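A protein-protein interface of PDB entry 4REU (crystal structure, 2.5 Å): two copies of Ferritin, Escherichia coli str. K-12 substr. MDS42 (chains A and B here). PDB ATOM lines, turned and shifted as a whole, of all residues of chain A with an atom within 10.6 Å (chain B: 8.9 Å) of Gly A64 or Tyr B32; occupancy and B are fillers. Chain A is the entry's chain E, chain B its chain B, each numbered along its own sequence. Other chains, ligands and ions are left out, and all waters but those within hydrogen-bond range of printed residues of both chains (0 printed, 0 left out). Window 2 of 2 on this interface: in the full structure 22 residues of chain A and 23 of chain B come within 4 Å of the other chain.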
ATOM      1  N   LEU A   1       2.465 -25.192  -8.995  1.00  0.00           N
ATOM      2  CA  LEU A   1       2.811 -24.059  -8.050  1.00  0.00           C
ATOM      3  C   LEU A   1       3.534 -24.571  -6.812  1.00  0.00           C
ATOM      4  O   LEU A   1       3.125 -25.582  -6.263  1.00  0.00           O
ATOM      5  CB  LEU A   1       1.549 -23.305  -7.587  1.00  0.00           C
ATOM      6  CG  LEU A   1       1.316 -21.865  -8.049  1.00  0.00           C
ATOM      7  CD1 LEU A   1       1.362 -21.781  -9.564  1.00  0.00           C
ATOM      8  CD2 LEU A   1      -0.024 -21.350  -7.548  1.00  0.00           C
ATOM      9  N   LYS A   2       4.572 -23.871  -6.354  1.00  0.00           N
ATOM     10  CA  LYS A   2       5.296 -24.313  -5.146  1.00  0.00           C
ATOM     11  C   LYS A   2       4.457 -24.079  -3.888  1.00  0.00           C
ATOM     12  O   LYS A   2       3.760 -23.096  -3.788  1.00  0.00           O
ATOM     13  CB  LYS A   2       6.657 -23.641  -5.027  1.00  0.00           C
ATOM     14  CG  LYS A   2       7.608 -24.066  -6.141  1.00  0.00           C
ATOM     15  CD  LYS A   2       9.061 -23.679  -5.878  1.00  0.00           C
ATOM     16  CE  LYS A   2       9.963 -24.076  -7.046  1.00  0.00           C
ATOM     17  NZ  LYS A   2      11.408 -23.807  -6.784  1.00  0.00           N
ATOM     18  N   ILE A   6       1.671 -21.030  -2.765  1.00  0.00           N
ATOM     19  CA  ILE A   6       0.261 -21.293  -2.470  1.00  0.00           C
ATOM     20  C   ILE A   6      -0.128 -20.711  -1.105  1.00  0.00           C
ATOM     21  O   ILE A   6      -1.105 -19.980  -0.981  1.00  0.00           O
ATOM     22  CB  ILE A   6      -0.041 -22.804  -2.500  1.00  0.00           C
ATOM     23  CG1 ILE A   6       0.108 -23.324  -3.936  1.00  0.00           C
ATOM     24  CG2 ILE A   6      -1.446 -23.090  -1.995  1.00  0.00           C
ATOM     25  CD1 ILE A   6       0.408 -24.801  -4.006  1.00  0.00           C
ATOM     26  N   LEU A   9      -0.003 -16.777  -1.343  1.00  0.00           N
ATOM     27  CA  LEU A   9      -1.057 -16.256  -2.146  1.00  0.00           C
ATOM     28  C   LEU A   9      -2.334 -16.337  -1.349  1.00  0.00           C
ATOM     29  O   LEU A   9      -3.128 -15.401  -1.327  1.00  0.00           O
ATOM     30  CB  LEU A   9      -1.175 -17.040  -3.442  1.00  0.00           C
ATOM     31  CG  LEU A   9      -0.120 -16.724  -4.497  1.00  0.00           C
ATOM     32  CD1 LEU A   9      -0.256 -17.704  -5.649  1.00  0.00           C
ATOM     33  CD2 LEU A   9      -0.226 -15.297  -5.018  1.00  0.00           C
ATOM     34  N   ASN A  10      -2.526 -17.467  -0.690  1.00  0.00           N
ATOM     35  CA  ASN A  10      -3.659 -17.627   0.206  1.00  0.00           C
ATOM     36  C   ASN A  10      -3.665 -16.616   1.385  1.00  0.00           C
ATOM     37  O   ASN A  10      -4.738 -16.123   1.772  1.00  0.00           O
ATOM     38  CB  ASN A  10      -3.764 -19.077   0.708  1.00  0.00           C
ATOM     39  CG  ASN A  10      -5.166 -19.430   1.188  1.00  0.00           C
ATOM     40  OD1 ASN A  10      -6.047 -19.699   0.378  1.00  0.00           O
ATOM     41  ND2 ASN A  10      -5.392 -19.378   2.503  1.00  0.00           N
ATOM     42  N   LEU A  56      -7.508 -13.022  -6.402  1.00  0.00           N
ATOM     43  CA  LEU A  56      -6.577 -14.001  -5.820  1.00  0.00           C
ATOM     44  C   LEU A  56      -7.267 -15.333  -5.644  1.00  0.00           C
ATOM     45  O   LEU A  56      -6.705 -16.386  -5.894  1.00  0.00           O
ATOM     46  CB  LEU A  56      -6.054 -13.510  -4.450  1.00  0.00           C
ATOM     47  CG  LEU A  56      -4.833 -12.578  -4.495  1.00  0.00           C
ATOM     48  CD1 LEU A  56      -4.884 -11.622  -3.327  1.00  0.00           C
ATOM     49  CD2 LEU A  56      -3.514 -13.342  -4.481  1.00  0.00           C
ATOM     50  N   PHE A  57      -8.504 -15.283  -5.195  1.00  0.00           N
ATOM     51  CA  PHE A  57      -9.345 -16.479  -5.125  1.00  0.00           C
ATOM     52  C   PHE A  57      -9.362 -17.180  -6.480  1.00  0.00           C
ATOM     53  O   PHE A  57      -9.047 -18.343  -6.570  1.00  0.00           O
ATOM     54  CB  PHE A  57     -10.748 -16.041  -4.749  1.00  0.00           C
ATOM     55  CG  PHE A  57     -11.566 -17.083  -4.063  1.00  0.00           C
ATOM     56  CD1 PHE A  57     -12.397 -17.919  -4.791  1.00  0.00           C
ATOM     57  CD2 PHE A  57     -11.560 -17.167  -2.689  1.00  0.00           C
ATOM     58  CE1 PHE A  57     -13.189 -18.835  -4.156  1.00  0.00           C
ATOM     59  CE2 PHE A  57     -12.328 -18.096  -2.051  1.00  0.00           C
ATOM     60  CZ  PHE A  57     -13.145 -18.934  -2.788  1.00  0.00           C
ATOM     61  N   ASP A  58      -9.669 -16.438  -7.539  1.00  0.00           N
ATOM     62  CA  ASP A  58      -9.695 -16.997  -8.881  1.00  0.00           C
ATOM     63  C   ASP A  58      -8.350 -17.560  -9.343  1.00  0.00           C
ATOM     64  O   ASP A  58      -8.324 -18.598  -9.976  1.00  0.00           O
ATOM     65  CB  ASP A  58     -10.178 -15.948  -9.893  1.00  0.00           C
ATOM     66  CG  ASP A  58     -11.628 -15.538  -9.687  1.00  0.00           C
ATOM     67  OD1 ASP A  58     -12.325 -16.181  -8.871  1.00  0.00           O
ATOM     68  OD2 ASP A  58     -12.069 -14.546 -10.327  1.00  0.00           O
ATOM     69  N   TYR A  59      -7.243 -16.879  -9.050  1.00  0.00           N
ATOM     70  CA  TYR A  59      -5.921 -17.372  -9.479  1.00  0.00           C
ATOM     71  C   TYR A  59      -5.602 -18.688  -8.813  1.00  0.00           C
ATOM     72  O   TYR A  59      -5.039 -19.592  -9.447  1.00  0.00           O
ATOM     73  CB  TYR A  59      -4.775 -16.361  -9.186  1.00  0.00           C
ATOM     74  CG  TYR A  59      -3.377 -16.806  -9.656  1.00  0.00           C
ATOM     75  CD1 TYR A  59      -2.994 -16.728 -11.014  1.00  0.00           C
ATOM     76  CD2 TYR A  59      -2.426 -17.273  -8.752  1.00  0.00           C
ATOM     77  CE1 TYR A  59      -1.714 -17.091 -11.432  1.00  0.00           C
ATOM     78  CE2 TYR A  59      -1.145 -17.656  -9.169  1.00  0.00           C
ATOM     79  CZ  TYR A  59      -0.793 -17.569 -10.508  1.00  0.00           C
ATOM     80  OH  TYR A  59       0.493 -17.952 -10.904  1.00  0.00           O
ATOM     81  N   LEU A  60      -5.931 -18.802  -7.532  1.00  0.00           N
ATOM     82  CA  LEU A  60      -5.694 -20.058  -6.816  1.00  0.00           C
ATOM     83  C   LEU A  60      -6.504 -21.170  -7.428  1.00  0.00           C
ATOM     84  O   LEU A  60      -6.001 -22.245  -7.645  1.00  0.00           O
ATOM     85  CB  LEU A  60      -6.022 -19.932  -5.328  1.00  0.00           C
ATOM     86  CG  LEU A  60      -4.966 -19.201  -4.498  1.00  0.00           C
ATOM     87  CD1 LEU A  60      -5.509 -18.861  -3.137  1.00  0.00           C
ATOM     88  CD2 LEU A  60      -3.673 -19.959  -4.317  1.00  0.00           C
ATOM     89  N   THR A  61      -7.757 -20.924  -7.741  1.00  0.00           N
ATOM     90  CA  THR A  61      -8.564 -22.008  -8.305  1.00  0.00           C
ATOM     91  C   THR A  61      -8.140 -22.347  -9.736  1.00  0.00           C
ATOM     92  O   THR A  61      -8.138 -23.516 -10.101  1.00  0.00           O
ATOM     93  CB  THR A  61     -10.089 -21.772  -8.228  1.00  0.00           C
ATOM     94  OG1 THR A  61     -10.455 -20.595  -8.942  1.00  0.00           O
ATOM     95  CG2 THR A  61     -10.529 -21.646  -6.778  1.00  0.00           C
ATOM     96  N   ASP A  62      -7.750 -21.332 -10.514  1.00  0.00           N
ATOM     97  CA  ASP A  62      -7.291 -21.537 -11.886  1.00  0.00           C
ATOM     98  C   ASP A  62      -6.053 -22.414 -11.867  1.00  0.00           C
ATOM     99  O   ASP A  62      -5.906 -23.250 -12.720  1.00  0.00           O
ATOM    100  CB  ASP A  62      -6.948 -20.229 -12.591  1.00  0.00           C
ATOM    101  CG  ASP A  62      -8.182 -19.341 -12.887  1.00  0.00           C
ATOM    102  OD1 ASP A  62      -9.365 -19.789 -12.780  1.00  0.00           O
ATOM    103  OD2 ASP A  62      -7.932 -18.151 -13.227  1.00  0.00           O
ATOM    104  N   THR A  63      -5.186 -22.251 -10.872  1.00  0.00           N
ATOM    105  CA  THR A  63      -3.962 -23.034 -10.800  1.00  0.00           C
ATOM    106  C   THR A  63      -4.128 -24.392 -10.155  1.00  0.00           C
ATOM    107  O   THR A  63      -3.131 -24.991  -9.761  1.00  0.00           O
ATOM    108  CB  THR A  63      -2.873 -22.304  -9.984  1.00  0.00           C
ATOM    109  OG1 THR A  63      -3.376 -21.959  -8.676  1.00  0.00           O
ATOM    110  CG2 THR A  63      -2.384 -21.070 -10.729  1.00  0.00           C
ATOM    111  N   GLY A  64      -5.367 -24.873 -10.011  1.00  0.00           N
ATOM    112  CA  GLY A  64      -5.617 -26.185  -9.413  1.00  0.00           C
ATOM    113  C   GLY A  64      -5.566 -26.272  -7.893  1.00  0.00           C
ATOM    114  O   GLY A  64      -5.539 -27.371  -7.328  1.00  0.00           O
ATOM    115  N   ASN A  65      -5.600 -25.127  -7.218  1.00  0.00           N
ATOM    116  CA  ASN A  65      -5.581 -25.099  -5.764  1.00  0.00           C
ATOM    117  C   ASN A  65      -6.897 -24.685  -5.181  1.00  0.00           C
ATOM    118  O   ASN A  65      -7.710 -24.039  -5.846  1.00  0.00           O
ATOM    119  CB  ASN A  65      -4.509 -24.162  -5.272  1.00  0.00           C
ATOM    120  CG  ASN A  65      -3.154 -24.566  -5.779  1.00  0.00           C
ATOM    121  OD1 ASN A  65      -2.547 -25.517  -5.263  1.00  0.00           O
ATOM    122  ND2 ASN A  65      -2.678 -23.873  -6.820  1.00  0.00           N
ATOM    123  N   LEU A  66      -7.087 -25.070  -3.925  1.00  0.00           N
ATOM    124  CA  LEU A  66      -8.295 -24.789  -3.186  1.00  0.00           C
ATOM    125  C   LEU A  66      -8.021 -23.631  -2.219  1.00  0.00           C
ATOM    126  O   LEU A  66      -7.326 -23.805  -1.205  1.00  0.00           O
ATOM    127  CB  LEU A  66      -8.732 -26.028  -2.438  1.00  0.00           C
ATOM    128  CG  LEU A  66     -10.000 -25.935  -1.597  1.00  0.00           C
ATOM    129  CD1 LEU A  66     -11.264 -25.949  -2.422  1.00  0.00           C
ATOM    130  CD2 LEU A  66      -9.974 -27.127  -0.657  1.00  0.00           C
ATOM    131  N   PRO A  67      -8.549 -22.433  -2.542  1.00  0.00           N
ATOM    132  CA  PRO A  67      -8.385 -21.352  -1.585  1.00  0.00           C
ATOM    133  C   PRO A  67      -9.163 -21.609  -0.296  1.00  0.00           C
ATOM    134  O   PRO A  67     -10.258 -22.165  -0.328  1.00  0.00           O
ATOM    135  CB  PRO A  67      -8.940 -20.142  -2.315  1.00  0.00           C
ATOM    136  CG  PRO A  67      -9.851 -20.691  -3.358  1.00  0.00           C
ATOM    137  CD  PRO A  67      -9.281 -22.012  -3.746  1.00  0.00           C
ATOM    138  N   ARG A  68      -8.568 -21.191   0.812  1.00  0.00           N
ATOM    139  CA  ARG A  68      -9.110 -21.346   2.140  1.00  0.00           C
ATOM    140  C   ARG A  68      -9.282 -20.005   2.839  1.00  0.00           C
ATOM    141  O   ARG A  68      -8.318 -19.340   3.225  1.00  0.00           O
ATOM    142  CB  ARG A  68      -8.187 -22.211   2.971  1.00  0.00           C
ATOM    143  CG  ARG A  68      -8.737 -22.577   4.335  1.00  0.00           C
ATOM    144  CD  ARG A  68      -7.815 -23.587   4.987  1.00  0.00           C
ATOM    145  NE  ARG A  68      -8.413 -24.298   6.117  1.00  0.00           N
ATOM    146  CZ  ARG A  68      -8.139 -25.569   6.426  1.00  0.00           C
ATOM    147  NH1 ARG A  68      -8.715 -26.144   7.490  1.00  0.00           N
ATOM    148  NH2 ARG A  68      -7.294 -26.284   5.668  1.00  0.00           N
ATOM    149  N   GLN B  25     -16.635 -19.732  -0.178  1.00  0.00           N
ATOM    150  CA  GLN B  25     -15.750 -20.843   0.059  1.00  0.00           C
ATOM    151  C   GLN B  25     -16.330 -22.052  -0.637  1.00  0.00           C
ATOM    152  O   GLN B  25     -15.611 -22.832  -1.252  1.00  0.00           O
ATOM    153  CB  GLN B  25     -15.663 -21.133   1.546  1.00  0.00           C
ATOM    154  CG  GLN B  25     -14.811 -22.321   1.933  1.00  0.00           C
ATOM    155  CD  GLN B  25     -13.346 -22.113   1.572  1.00  0.00           C
ATOM    156  OE1 GLN B  25     -12.807 -22.696   0.607  1.00  0.00           O
ATOM    157  NE2 GLN B  25     -12.702 -21.271   2.327  1.00  0.00           N
ATOM    158  N   MET B  26     -17.641 -22.220  -0.532  1.00  0.00           N
ATOM    159  CA  MET B  26     -18.275 -23.347  -1.181  1.00  0.00           C
ATOM    160  C   MET B  26     -18.094 -23.298  -2.698  1.00  0.00           C
ATOM    161  O   MET B  26     -17.933 -24.330  -3.349  1.00  0.00           O
ATOM    162  CB  MET B  26     -19.746 -23.367  -0.844  1.00  0.00           C
ATOM    163  CG  MET B  26     -20.093 -23.950   0.504  1.00  0.00           C
ATOM    164  SD  MET B  26     -21.855 -23.657   0.722  1.00  0.00           S
ATOM    165  CE  MET B  26     -22.135 -24.849   2.021  1.00  0.00           C
ATOM    166  N   SER B  27     -18.105 -22.096  -3.263  1.00  0.00           N
ATOM    167  CA  SER B  27     -17.871 -21.972  -4.697  1.00  0.00           C
ATOM    168  C   SER B  27     -16.473 -22.492  -5.052  1.00  0.00           C
ATOM    169  O   SER B  27     -16.263 -23.034  -6.130  1.00  0.00           O
ATOM    170  CB  SER B  27     -18.060 -20.540  -5.203  1.00  0.00           C
ATOM    171  OG  SER B  27     -16.837 -19.864  -5.189  1.00  0.00           O
ATOM    172  N   ALA B  28     -15.529 -22.324  -4.137  1.00  0.00           N
ATOM    173  CA  ALA B  28     -14.153 -22.803  -4.347  1.00  0.00           C
ATOM    174  C   ALA B  28     -14.085 -24.316  -4.458  1.00  0.00           C
ATOM    175  O   ALA B  28     -13.464 -24.834  -5.360  1.00  0.00           O
ATOM    176  CB  ALA B  28     -13.246 -22.335  -3.218  1.00  0.00           C
ATOM    177  N   TRP B  29     -14.718 -24.992  -3.505  1.00  0.00           N
ATOM    178  CA  TRP B  29     -14.911 -26.431  -3.524  1.00  0.00           C
ATOM    179  C   TRP B  29     -15.522 -26.879  -4.825  1.00  0.00           C
ATOM    180  O   TRP B  29     -15.116 -27.867  -5.385  1.00  0.00           O
ATOM    181  CB  TRP B  29     -15.864 -26.861  -2.413  1.00  0.00           C
ATOM    182  CG  TRP B  29     -15.974 -28.362  -2.288  1.00  0.00           C
ATOM    183  CD1 TRP B  29     -15.264 -29.179  -1.424  1.00  0.00           C
ATOM    184  CD2 TRP B  29     -16.811 -29.233  -3.064  1.00  0.00           C
ATOM    185  NE1 TRP B  29     -15.638 -30.495  -1.608  1.00  0.00           N
ATOM    186  CE2 TRP B  29     -16.579 -30.551  -2.611  1.00  0.00           C
ATOM    187  CE3 TRP B  29     -17.741 -29.027  -4.098  1.00  0.00           C
ATOM    188  CZ2 TRP B  29     -17.244 -31.650  -3.157  1.00  0.00           C
ATOM    189  CZ3 TRP B  29     -18.414 -30.142  -4.637  1.00  0.00           C
ATOM    190  CH2 TRP B  29     -18.161 -31.415  -4.171  1.00  0.00           C
ATOM    191  N   CYS B  30     -16.542 -26.174  -5.276  1.00  0.00           N
ATOM    192  CA  CYS B  30     -17.159 -26.499  -6.534  1.00  0.00           C
ATOM    193  C   CYS B  30     -16.092 -26.459  -7.639  1.00  0.00           C
ATOM    194  O   CYS B  30     -15.884 -27.455  -8.318  1.00  0.00           O
ATOM    195  CB  CYS B  30     -18.374 -25.593  -6.799  1.00  0.00           C
ATOM    196  SG  CYS B  30     -19.829 -26.058  -5.810  1.00  0.00           S
ATOM    197  N   SER B  31     -15.370 -25.350  -7.768  1.00  0.00           N
ATOM    198  CA  SER B  31     -14.396 -25.187  -8.852  1.00  0.00           C
ATOM    199  C   SER B  31     -13.325 -26.278  -8.803  1.00  0.00           C
ATOM    200  O   SER B  31     -13.025 -26.896  -9.807  1.00  0.00           O
ATOM    201  CB  SER B  31     -13.766 -23.791  -8.809  1.00  0.00           C
ATOM    202  OG  SER B  31     -14.639 -22.821  -9.361  1.00  0.00           O
ATOM    203  N   TYR B  32     -12.780 -26.528  -7.626  1.00  0.00           N
ATOM    204  CA  TYR B  32     -11.792 -27.588  -7.401  1.00  0.00           C
ATOM    205  C   TYR B  32     -12.264 -28.997  -7.759  1.00  0.00           C
ATOM    206  O   TYR B  32     -11.429 -29.868  -7.972  1.00  0.00           O
ATOM    207  CB  TYR B  32     -11.393 -27.580  -5.929  1.00  0.00           C
ATOM    208  CG  TYR B  32     -10.245 -28.472  -5.553  1.00  0.00           C
ATOM    209  CD1 TYR B  32      -8.965 -28.218  -6.033  1.00  0.00           C
ATOM    210  CD2 TYR B  32     -10.412 -29.539  -4.660  1.00  0.00           C
ATOM    211  CE1 TYR B  32      -7.883 -29.020  -5.685  1.00  0.00           C
ATOM    212  CE2 TYR B  32      -9.328 -30.353  -4.301  1.00  0.00           C
ATOM    213  CZ  TYR B  32      -8.064 -30.082  -4.827  1.00  0.00           C
ATOM    214  OH  TYR B  32      -6.970 -30.834  -4.509  1.00  0.00           O
ATOM    215  N   HIS B  33     -13.587 -29.229  -7.777  1.00  0.00           N
ATOM    216  CA  HIS B  33     -14.186 -30.535  -8.168  1.00  0.00           C
ATOM    217  C   HIS B  33     -14.942 -30.433  -9.507  1.00  0.00           C
ATOM    218  O   HIS B  33     -15.791 -31.258  -9.808  1.00  0.00           O
ATOM    219  CB  HIS B  33     -15.095 -31.126  -7.050  1.00  0.00           C
ATOM    220  CG  HIS B  33     -14.344 -31.727  -5.884  1.00  0.00           C
ATOM    221  ND1 HIS B  33     -14.068 -31.017  -4.736  1.00  0.00           N
ATOM    222  CD2 HIS B  33     -13.840 -32.974  -5.678  1.00  0.00           C
ATOM    223  CE1 HIS B  33     -13.411 -31.788  -3.883  1.00  0.00           C
ATOM    224  NE2 HIS B  33     -13.257 -32.982  -4.427  1.00  0.00           N
ATOM    225  N   THR B  34     -14.608 -29.411 -10.293  1.00  0.00           N
ATOM    226  CA  THR B  34     -15.044 -29.219 -11.710  1.00  0.00           C
ATOM    227  C   THR B  34     -16.469 -28.681 -11.968  1.00  0.00           C
ATOM    228  O   THR B  34     -16.897 -28.589 -13.121  1.00  0.00           O
ATOM    229  CB  THR B  34     -14.799 -30.472 -12.605  1.00  0.00           C
ATOM    230  OG1 THR B  34     -15.831 -31.442 -12.389  1.00  0.00           O
ATOM    231  CG2 THR B  34     -13.405 -31.117 -12.333  1.00  0.00           C
ATOM    232  N   PHE B  35     -17.196 -28.315 -10.916  1.00  0.00           N
ATOM    233  CA  PHE B  35     -18.575 -27.815 -11.074  1.00  0.00           C
ATOM    234  C   PHE B  35     -18.578 -26.302 -11.234  1.00  0.00           C
ATOM    235  O   PHE B  35     -18.839 -25.556 -10.303  1.00  0.00           O
ATOM    236  CB  PHE B  35     -19.432 -28.224  -9.895  1.00  0.00           C
ATOM    237  CG  PHE B  35     -19.354 -29.680  -9.575  1.00  0.00           C
ATOM    238  CD1 PHE B  35     -19.970 -30.624 -10.399  1.00  0.00           C
ATOM    239  CD2 PHE B  35     -18.692 -30.123  -8.435  1.00  0.00           C
ATOM    240  CE1 PHE B  35     -19.909 -31.984 -10.086  1.00  0.00           C
ATOM    241  CE2 PHE B  35     -18.636 -31.481  -8.113  1.00  0.00           C
ATOM    242  CZ  PHE B  35     -19.237 -32.409  -8.942  1.00  0.00           C
ATOM    243  N   GLU B  36     -18.271 -25.866 -12.438  1.00  0.00           N
ATOM    244  CA  GLU B  36     -18.052 -24.464 -12.708  1.00  0.00           C
ATOM    245  C   GLU B  36     -19.357 -23.680 -12.598  1.00  0.00           C
ATOM    246  O   GLU B  36     -19.350 -22.500 -12.300  1.00  0.00           O
ATOM    247  CB  GLU B  36     -17.395 -24.285 -14.108  1.00  0.00           C
ATOM    248  CG  GLU B  36     -15.952 -23.733 -14.162  1.00  0.00           C
ATOM    249  CD  GLU B  36     -15.057 -24.079 -12.959  1.00  0.00           C
ATOM    250  OE1 GLU B  36     -14.748 -23.153 -12.166  1.00  0.00           O
ATOM    251  OE2 GLU B  36     -14.643 -25.251 -12.811  1.00  0.00           O
ATOM    252  N   ALA B  39     -20.244 -23.266  -8.839  1.00  0.00           N
ATOM    253  CA  ALA B  39     -19.331 -22.194  -8.416  1.00  0.00           C
ATOM    254  C   ALA B  39     -19.804 -20.807  -8.836  1.00  0.00           C
ATOM    255  O   ALA B  39     -19.724 -19.864  -8.069  1.00  0.00           O
ATOM    256  CB  ALA B  39     -17.931 -22.442  -8.943  1.00  0.00           C
ATOM    257  N   ARG B  43     -20.911 -17.934  -6.063  1.00  0.00           N
ATOM    258  CA  ARG B  43     -20.207 -16.673  -6.146  1.00  0.00           C
ATOM    259  C   ARG B  43     -21.233 -15.528  -6.281  1.00  0.00           C
ATOM    260  O   ARG B  43     -21.160 -14.539  -5.558  1.00  0.00           O
ATOM    261  CB  ARG B  43     -19.192 -16.767  -7.288  1.00  0.00           C
ATOM    262  CG  ARG B  43     -18.405 -15.514  -7.679  1.00  0.00           C
ATOM    263  CD  ARG B  43     -17.657 -15.774  -9.010  1.00  0.00           C
ATOM    264  NE  ARG B  43     -16.985 -17.094  -8.982  1.00  0.00           N
ATOM    265  CZ  ARG B  43     -16.964 -18.011  -9.968  1.00  0.00           C
ATOM    266  NH1 ARG B  43     -16.315 -19.153  -9.762  1.00  0.00           N
ATOM    267  NH2 ARG B  43     -17.573 -17.818 -11.141  1.00  0.00           N
ATOM    268  N   PHE B  76     -14.350 -22.952   6.192  1.00  0.00           N
ATOM    269  CA  PHE B  76     -13.827 -24.108   5.503  1.00  0.00           C
ATOM    270  C   PHE B  76     -14.471 -25.418   5.981  1.00  0.00           C
ATOM    271  O   PHE B  76     -14.583 -25.672   7.177  1.00  0.00           O
ATOM    272  CB  PHE B  76     -12.307 -24.197   5.665  1.00  0.00           C
ATOM    273  CG  PHE B  76     -11.677 -25.245   4.787  1.00  0.00           C
ATOM    274  CD1 PHE B  76     -11.296 -24.941   3.476  1.00  0.00           C
ATOM    275  CD2 PHE B  76     -11.493 -26.542   5.250  1.00  0.00           C
ATOM    276  CE1 PHE B  76     -10.717 -25.903   2.658  1.00  0.00           C
ATOM    277  CE2 PHE B  76     -10.924 -27.505   4.436  1.00  0.00           C
ATOM    278  CZ  PHE B  76     -10.529 -27.185   3.143  1.00  0.00           C
ATOM    279  N   GLU B  78     -14.931 -29.858   4.592  1.00  0.00           N
ATOM    280  CA  GLU B  78     -14.843 -30.954   3.633  1.00  0.00           C
ATOM    281  C   GLU B  78     -16.265 -31.382   3.285  1.00  0.00           C
ATOM    282  O   GLU B  78     -17.098 -31.573   4.159  1.00  0.00           O
ATOM    283  CB  GLU B  78     -14.069 -32.145   4.225  1.00  0.00           C
ATOM    284  CG  GLU B  78     -12.566 -31.918   4.438  1.00  0.00           C
ATOM    285  CD  GLU B  78     -11.718 -32.005   3.151  1.00  0.00           C
ATOM    286  OE1 GLU B  78     -11.902 -31.164   2.237  1.00  0.00           O
ATOM    287  OE2 GLU B  78     -10.834 -32.899   3.053  1.00  0.00           O
ATOM    288  N   TYR B  79     -16.540 -31.514   2.001  1.00  0.00           N
ATOM    289  CA  TYR B  79     -17.817 -32.010   1.537  1.00  0.00           C
ATOM    290  C   TYR B  79     -17.612 -33.271   0.688  1.00  0.00           C
ATOM    291  O   TYR B  79     -16.826 -33.249  -0.275  1.00  0.00           O
ATOM    292  CB  TYR B  79     -18.538 -30.962   0.680  1.00  0.00           C
ATOM    293  CG  TYR B  79     -18.795 -29.656   1.364  1.00  0.00           C
ATOM    294  CD1 TYR B  79     -19.714 -29.564   2.410  1.00  0.00           C
ATOM    295  CD2 TYR B  79     -18.130 -28.497   0.955  1.00  0.00           C
ATOM    296  CE1 TYR B  79     -19.950 -28.357   3.043  1.00  0.00           C
ATOM    297  CE2 TYR B  79     -18.361 -27.283   1.573  1.00  0.00           C
ATOM    298  CZ  TYR B  79     -19.267 -27.215   2.624  1.00  0.00           C
ATOM    299  OH  TYR B  79     -19.495 -26.008   3.231  1.00  0.00           O
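Of the printed residues of chain B, Phe A57 touches Ser B27 (3.9 Å) and Ala B28 (3.4 Å).
Of chain B, only Tyr B32 comes within 4 Å of Gly A64.
No residue of chain B comes within 4 Å of Asn A65.
Printed residues of chain B within 4 Å of Leu A66: Ala B28 (3.8 Å), Trp B29 (3.7 Å), Tyr B32 (3.9 Å) and Phe B76 (3.6 Å).
Of the printed residues of chain B, Pro A67 touches Gln B25 (2.8 Å) and Ala B28 (3.8 Å).
Of the printed residues of chain B, Arg A68 touches Gln B25 and Phe B76.
Of the printed residues of chain A, Ser B27 touches Phe A57.
Of chain A, only Phe A57, Leu A66 and Pro A67 come within 4 Å of Ala B28.
Of the printed residues of chain A, Tyr B32 touches Gly A64 (3.3 Å) and Leu A66 (3.9 Å).
No residue of chain A comes within 4 Å of His B33.
The nearest residue of chain B that does not touch Gly A64 is Ser B31 (7.5 Å).
The nearest residue of chain A that does not touch Tyr B32 is Asn A65 (4.2 Å).
No position is printed for both chains.
OD1 of Asn A10 lies within hydrogen-bond range of N of Arg A68 (3.0 Å).
The indole nitrogen of Trp B29 is in hydrogen-bond range of the backbone carbonyl oxygen of Tyr B79, at 3.3 Å.
O of Trp B29 sits close to ND1 of His B33 (3.4 Å).
The side-chain amide oxygen (OE1) of Gln B25 lies close to the backbone carbonyl oxygen (O) of Pro A67, at 2.8 Å.
Hydrophobic or aromatic side chains of chain A that line the printed part of chain B: Phe A57, Leu A66 and Pro A67.
Of the 17 printed residues of chain B, 6 touch a printed residue of chain A.
Printed residues of chain B that touch a printed residue of chain A: Gln B25, Ser B27, Ala B28, Trp B29, Tyr B32 and Phe B76.
Among the printed residues, 11 pairs touch across the chains.
Ser B27 touches Phe A57.
Phe A57 touches Ala B28 (CZ to CB, 3.4 Å).
Gly A64 touches Tyr B32.
CD1 of Leu A66 touches O of Ala B28, 3.8 Å away.
Trp B29 touches Leu A66 (N to CD1, 3.7 Å).
Leu A66 touches Tyr B32.
Leu A66 touches Phe B76 (CD2 to CE1, 3.6 Å).
CB of Ala B28 touches CG of Pro A67, at 3.8 Å.
NE2 of Gln B25 touches CA of Arg A68, 3.6 Å away.
Phe B76 touches Arg A68 (CD1 to CG, 3.6 Å).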
